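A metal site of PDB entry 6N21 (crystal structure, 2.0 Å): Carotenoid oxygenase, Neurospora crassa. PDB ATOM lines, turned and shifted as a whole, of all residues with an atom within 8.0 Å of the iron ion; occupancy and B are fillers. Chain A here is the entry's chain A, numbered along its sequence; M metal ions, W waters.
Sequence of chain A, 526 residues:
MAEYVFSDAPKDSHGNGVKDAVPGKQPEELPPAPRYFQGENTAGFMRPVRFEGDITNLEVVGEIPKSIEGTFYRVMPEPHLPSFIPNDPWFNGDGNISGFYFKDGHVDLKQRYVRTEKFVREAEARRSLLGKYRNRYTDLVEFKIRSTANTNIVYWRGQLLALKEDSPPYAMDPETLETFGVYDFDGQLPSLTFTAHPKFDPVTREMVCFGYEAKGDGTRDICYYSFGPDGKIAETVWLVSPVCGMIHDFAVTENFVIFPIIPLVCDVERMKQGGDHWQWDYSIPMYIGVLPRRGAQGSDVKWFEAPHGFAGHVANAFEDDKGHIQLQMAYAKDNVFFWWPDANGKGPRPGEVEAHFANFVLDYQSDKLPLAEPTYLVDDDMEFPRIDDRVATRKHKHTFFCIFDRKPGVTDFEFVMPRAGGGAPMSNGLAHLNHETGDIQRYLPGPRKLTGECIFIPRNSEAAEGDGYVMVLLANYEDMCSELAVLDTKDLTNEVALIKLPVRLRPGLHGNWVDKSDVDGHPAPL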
ATOM      1  N   PHE A  91     -12.561   6.319  31.015  1.00  0.00           N
ATOM      2  CA  PHE A  91     -12.222   6.471  29.573  1.00  0.00           C
ATOM      3  C   PHE A  91     -13.371   7.068  28.736  1.00  0.00           C
ATOM      4  O   PHE A  91     -13.148   7.320  27.545  1.00  0.00           O
ATOM      5  CB  PHE A  91     -11.864   5.109  28.936  1.00  0.00           C
ATOM      6  CG  PHE A  91     -10.581   4.436  29.385  1.00  0.00           C
ATOM      7  CD1 PHE A  91      -9.649   5.082  30.193  1.00  0.00           C
ATOM      8  CD2 PHE A  91     -10.293   3.147  28.952  1.00  0.00           C
ATOM      9  CE1 PHE A  91      -8.475   4.437  30.581  1.00  0.00           C
ATOM     10  CE2 PHE A  91      -9.119   2.502  29.340  1.00  0.00           C
ATOM     11  CZ  PHE A  91      -8.225   3.154  30.173  1.00  0.00           C
ATOM     12  N   THR A 151      -7.715  11.134  25.253  1.00  0.00           N
ATOM     13  CA  THR A 151      -6.650  10.132  25.529  1.00  0.00           C
ATOM     14  C   THR A 151      -5.264  10.771  25.385  1.00  0.00           C
ATOM     15  O   THR A 151      -4.410  10.559  26.280  1.00  0.00           O
ATOM     16  CB  THR A 151      -6.755   8.912  24.601  1.00  0.00           C
ATOM     17  OG1 THR A 151      -8.089   8.404  24.674  1.00  0.00           O
ATOM     18  CG2 THR A 151      -5.776   7.822  24.979  1.00  0.00           C
ATOM     19  N   ASN A 152      -5.030  11.506  24.313  1.00  0.00           N
ATOM     20  CA  ASN A 152      -3.715  12.154  24.090  1.00  0.00           C
ATOM     21  C   ASN A 152      -3.930  13.486  23.386  1.00  0.00           C
ATOM     22  O   ASN A 152      -4.977  13.678  22.723  1.00  0.00           O
ATOM     23  CB  ASN A 152      -2.744  11.221  23.344  1.00  0.00           C
ATOM     24  CG  ASN A 152      -1.288  11.533  23.547  1.00  0.00           C
ATOM     25  OD1 ASN A 152      -0.923  12.515  24.213  1.00  0.00           O
ATOM     26  ND2 ASN A 152      -0.441  10.754  22.881  1.00  0.00           N
ATOM     27  N   GLU A 165      -8.867   6.641  20.003  1.00  0.00           N
ATOM     28  CA  GLU A 165      -8.473   5.566  19.060  1.00  0.00           C
ATOM     29  C   GLU A 165      -9.676   5.006  18.290  1.00  0.00           C
ATOM     30  O   GLU A 165      -9.452   4.181  17.394  1.00  0.00           O
ATOM     31  CB  GLU A 165      -7.707   4.485  19.828  1.00  0.00           C
ATOM     32  CG  GLU A 165      -8.556   3.685  20.804  1.00  0.00           C
ATOM     33  CD  GLU A 165      -7.709   2.933  21.829  1.00  0.00           C
ATOM     34  OE1 GLU A 165      -7.929   1.712  22.012  1.00  0.00           O
ATOM     35  OE2 GLU A 165      -6.825   3.573  22.451  1.00  0.00           O
ATOM     36  N   THR A 195      -4.845   6.225  16.070  1.00  0.00           N
ATOM     37  CA  THR A 195      -4.297   5.819  17.374  1.00  0.00           C
ATOM     38  C   THR A 195      -4.067   7.030  18.284  1.00  0.00           C
ATOM     39  O   THR A 195      -3.708   8.128  17.798  1.00  0.00           O
ATOM     40  CB  THR A 195      -2.979   5.062  17.202  1.00  0.00           C
ATOM     41  OG1 THR A 195      -2.545   4.628  18.489  1.00  0.00           O
ATOM     42  CG2 THR A 195      -1.916   5.917  16.546  1.00  0.00           C
ATOM     43  N   ALA A 196      -4.172   6.812  19.598  1.00  0.00           N
ATOM     44  CA  ALA A 196      -3.808   7.815  20.612  1.00  0.00           C
ATOM     45  C   ALA A 196      -2.276   7.897  20.747  1.00  0.00           C
ATOM     46  O   ALA A 196      -1.812   8.794  21.462  1.00  0.00           O
ATOM     47  CB  ALA A 196      -4.471   7.483  21.910  1.00  0.00           C
ATOM     48  N   HIS A 197      -1.518   7.000  20.120  1.00  0.00           N
ATOM     49  CA  HIS A 197      -0.045   6.918  20.328  1.00  0.00           C
ATOM     50  C   HIS A 197       0.699   6.907  19.006  1.00  0.00           C
ATOM     51  O   HIS A 197       1.460   5.976  18.734  1.00  0.00           O
ATOM     52  CB  HIS A 197       0.276   5.696  21.184  1.00  0.00           C
ATOM     53  CG  HIS A 197      -0.222   5.865  22.572  1.00  0.00           C
ATOM     54  ND1 HIS A 197       0.337   6.790  23.412  1.00  0.00           N
ATOM     55  CD2 HIS A 197      -1.248   5.287  23.234  1.00  0.00           C
ATOM     56  CE1 HIS A 197      -0.326   6.786  24.556  1.00  0.00           C
ATOM     57  NE2 HIS A 197      -1.294   5.854  24.480  1.00  0.00           N
ATOM     58  N   HIS A 248      -3.897  -0.591  21.513  1.00  0.00           N
ATOM     59  CA  HIS A 248      -3.876   0.734  22.178  1.00  0.00           C
ATOM     60  C   HIS A 248      -2.611   1.496  21.802  1.00  0.00           C
ATOM     61  O   HIS A 248      -2.687   2.754  21.618  1.00  0.00           O
ATOM     62  CB  HIS A 248      -3.942   0.581  23.693  1.00  0.00           C
ATOM     63  CG  HIS A 248      -3.893   1.920  24.341  1.00  0.00           C
ATOM     64  ND1 HIS A 248      -4.888   2.859  24.109  1.00  0.00           N
ATOM     65  CD2 HIS A 248      -2.961   2.512  25.115  1.00  0.00           C
ATOM     66  CE1 HIS A 248      -4.594   3.959  24.766  1.00  0.00           C
ATOM     67  NE2 HIS A 248      -3.418   3.777  25.373  1.00  0.00           N
ATOM     68  N   ASP A 249      -1.488   0.799  21.747  1.00  0.00           N
ATOM     69  CA  ASP A 249      -0.175   1.435  21.504  1.00  0.00           C
ATOM     70  C   ASP A 249       0.520   0.621  20.427  1.00  0.00           C
ATOM     71  O   ASP A 249       0.006  -0.447  20.061  1.00  0.00           O
ATOM     72  CB  ASP A 249       0.610   1.541  22.805  1.00  0.00           C
ATOM     73  CG  ASP A 249       1.674   2.623  22.840  1.00  0.00           C
ATOM     74  OD1 ASP A 249       2.091   3.089  21.755  1.00  0.00           O
ATOM     75  OD2 ASP A 249       2.111   2.970  23.958  1.00  0.00           O
ATOM     76  N   GLY A 312       0.692  -3.089  27.904  1.00  0.00           N
ATOM     77  CA  GLY A 312       0.687  -1.709  28.400  1.00  0.00           C
ATOM     78  C   GLY A 312       1.404  -0.780  27.434  1.00  0.00           C
ATOM     79  O   GLY A 312       1.663  -1.188  26.272  1.00  0.00           O
ATOM     80  N   HIS A 313       1.699   0.438  27.862  1.00  0.00           N
ATOM     81  CA  HIS A 313       2.289   1.472  26.978  1.00  0.00           C
ATOM     82  C   HIS A 313       3.707   1.086  26.570  1.00  0.00           C
ATOM     83  O   HIS A 313       4.450   0.522  27.389  1.00  0.00           O
ATOM     84  CB  HIS A 313       2.267   2.832  27.661  1.00  0.00           C
ATOM     85  CG  HIS A 313       0.880   3.346  27.786  1.00  0.00           C
ATOM     86  ND1 HIS A 313       0.212   3.351  28.987  1.00  0.00           N
ATOM     87  CD2 HIS A 313       0.034   3.813  26.851  1.00  0.00           C
ATOM     88  CE1 HIS A 313      -1.016   3.803  28.800  1.00  0.00           C
ATOM     89  NE2 HIS A 313      -1.144   4.088  27.507  1.00  0.00           N
ATOM     90  N   VAL A 314       4.057   1.412  25.338  1.00  0.00           N
ATOM     91  CA  VAL A 314       5.412   1.238  24.777  1.00  0.00           C
ATOM     92  C   VAL A 314       6.292   2.391  25.277  1.00  0.00           C
ATOM     93  O   VAL A 314       5.875   3.551  25.155  1.00  0.00           O
ATOM     94  CB  VAL A 314       5.351   1.197  23.241  1.00  0.00           C
ATOM     95  CG1 VAL A 314       6.737   1.184  22.632  1.00  0.00           C
ATOM     96  CG2 VAL A 314       4.485   0.036  22.769  1.00  0.00           C
ATOM     97  N   PHE A 337      -7.520  -3.926  32.603  1.00  0.00           N
ATOM     98  CA  PHE A 337      -8.862  -3.323  32.424  1.00  0.00           C
ATOM     99  C   PHE A 337      -9.921  -4.319  32.940  1.00  0.00           C
ATOM    100  O   PHE A 337     -10.750  -4.826  32.169  1.00  0.00           O
ATOM    101  CB  PHE A 337      -9.056  -2.887  30.972  1.00  0.00           C
ATOM    102  CG  PHE A 337      -8.090  -1.858  30.428  1.00  0.00           C
ATOM    103  CD1 PHE A 337      -7.258  -1.109  31.245  1.00  0.00           C
ATOM    104  CD2 PHE A 337      -8.046  -1.598  29.063  1.00  0.00           C
ATOM    105  CE1 PHE A 337      -6.399  -0.161  30.720  1.00  0.00           C
ATOM    106  CE2 PHE A 337      -7.200  -0.641  28.525  1.00  0.00           C
ATOM    107  CZ  PHE A 337      -6.362   0.066  29.356  1.00  0.00           C
ATOM    108  N   GLU A 383       4.028   2.037  34.865  1.00  0.00           N
ATOM    109  CA  GLU A 383       3.296   2.363  33.609  1.00  0.00           C
ATOM    110  C   GLU A 383       3.690   3.778  33.156  1.00  0.00           C
ATOM    111  O   GLU A 383       4.539   4.413  33.838  1.00  0.00           O
ATOM    112  CB  GLU A 383       1.783   2.222  33.828  1.00  0.00           C
ATOM    113  CG  GLU A 383       1.153   1.088  33.012  1.00  0.00           C
ATOM    114  CD  GLU A 383       1.118   1.295  31.506  1.00  0.00           C
ATOM    115  OE1 GLU A 383       1.452   2.416  31.057  1.00  0.00           O
ATOM    116  OE2 GLU A 383       0.773   0.344  30.795  1.00  0.00           O
ATOM    117  N   PHE A 384       3.118   4.247  32.053  1.00  0.00           N
ATOM    118  CA  PHE A 384       3.276   5.622  31.510  1.00  0.00           C
ATOM    119  C   PHE A 384       4.769   5.920  31.319  1.00  0.00           C
ATOM    120  O   PHE A 384       5.287   6.909  31.828  1.00  0.00           O
ATOM    121  CB  PHE A 384       2.554   6.629  32.402  1.00  0.00           C
ATOM    122  CG  PHE A 384       1.060   6.418  32.421  1.00  0.00           C
ATOM    123  CD1 PHE A 384       0.291   6.760  31.317  1.00  0.00           C
ATOM    124  CD2 PHE A 384       0.433   5.811  33.508  1.00  0.00           C
ATOM    125  CE1 PHE A 384      -1.073   6.535  31.311  1.00  0.00           C
ATOM    126  CE2 PHE A 384      -0.932   5.585  33.487  1.00  0.00           C
ATOM    127  CZ  PHE A 384      -1.678   5.934  32.381  1.00  0.00           C
ATOM    128  N   GLU A 453       1.116  11.038  34.350  1.00  0.00           N
ATOM    129  CA  GLU A 453       2.214  10.797  33.381  1.00  0.00           C
ATOM    130  C   GLU A 453       3.108  12.028  33.324  1.00  0.00           C
ATOM    131  O   GLU A 453       2.590  13.157  33.249  1.00  0.00           O
ATOM    132  CB  GLU A 453       1.668  10.511  31.996  1.00  0.00           C
ATOM    133  CG  GLU A 453       2.742  10.294  30.944  1.00  0.00           C
ATOM    134  CD  GLU A 453       2.178  10.322  29.535  1.00  0.00           C
ATOM    135  OE1 GLU A 453       1.656  11.412  29.134  1.00  0.00           O
ATOM    136  OE2 GLU A 453       2.239   9.263  28.857  1.00  0.00           O
ATOM    137  N   LEU A 509      -4.902  11.426  31.336  1.00  0.00           N
ATOM    138  CA  LEU A 509      -4.122  10.435  30.567  1.00  0.00           C
ATOM    139  C   LEU A 509      -2.882  11.167  30.058  1.00  0.00           C
ATOM    140  O   LEU A 509      -2.109  11.661  30.921  1.00  0.00           O
ATOM    141  CB  LEU A 509      -5.042   9.845  29.493  1.00  0.00           C
ATOM    142  CG  LEU A 509      -6.099   8.890  30.065  1.00  0.00           C
ATOM    143  CD1 LEU A 509      -7.249   8.651  29.086  1.00  0.00           C
ATOM    144  CD2 LEU A 509      -5.452   7.579  30.493  1.00  0.00           C
ATOM    145  N   HIS A 510      -2.674  11.204  28.759  1.00  0.00           N
ATOM    146  CA  HIS A 510      -1.373  11.551  28.173  1.00  0.00           C
ATOM    147  C   HIS A 510      -1.213  13.061  28.019  1.00  0.00           C
ATOM    148  O   HIS A 510      -2.224  13.817  28.004  1.00  0.00           O
ATOM    149  CB  HIS A 510      -1.178  10.776  26.881  1.00  0.00           C
ATOM    150  CG  HIS A 510      -1.176   9.313  27.125  1.00  0.00           C
ATOM    151  ND1 HIS A 510      -0.094   8.668  27.707  1.00  0.00           N
ATOM    152  CD2 HIS A 510      -2.123   8.378  26.905  1.00  0.00           C
ATOM    153  CE1 HIS A 510      -0.381   7.379  27.820  1.00  0.00           C
ATOM    154  NE2 HIS A 510      -1.614   7.199  27.337  1.00  0.00           N
HETATM  155 FE    FE M   1      -2.500   5.441  26.393  1.00  0.00          FE
HETATM  156  O   HOH W   1      -4.678   5.071  27.903  1.00  0.00           O
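The side-chain carboxylate of Glu 383 sits at hydrogen-bond distance from a ring nitrogen (ND1) of His 313 (2.6 Å). O of Thr 151 is in hydrogen-bond range of N of His 510 (3.1 Å). The backbone NH of His 197 sits at hydrogen-bond distance from the side-chain hydroxyl of Thr 195 (3.1 Å). A ring nitrogen (ND1) of His 510 is in hydrogen-bond range of the side-chain carboxylate of Glu 453, at 2.7 Å. The side-chain carboxylate (OE2) of Glu 165 lies within hydrogen-bond range of a ring nitrogen (ND1) of His 248, 2.6 Å away.
Within 4 Å of the iron ion: His 197, His 248, His 313 and His 510.
The iron ion is bound by a ring nitrogen (NE2) of His 248 (2.2 Å), a ring nitrogen (NE2) of His 510 (2.2 Å), a ring nitrogen (NE2) of His 313 (2.2 Å) and a ring nitrogen (NE2) of His 197 (2.3 Å). The iron ion has four donor atoms within binding distance. Slightly farther from the iron ion lies water W1 (2.7 Å).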
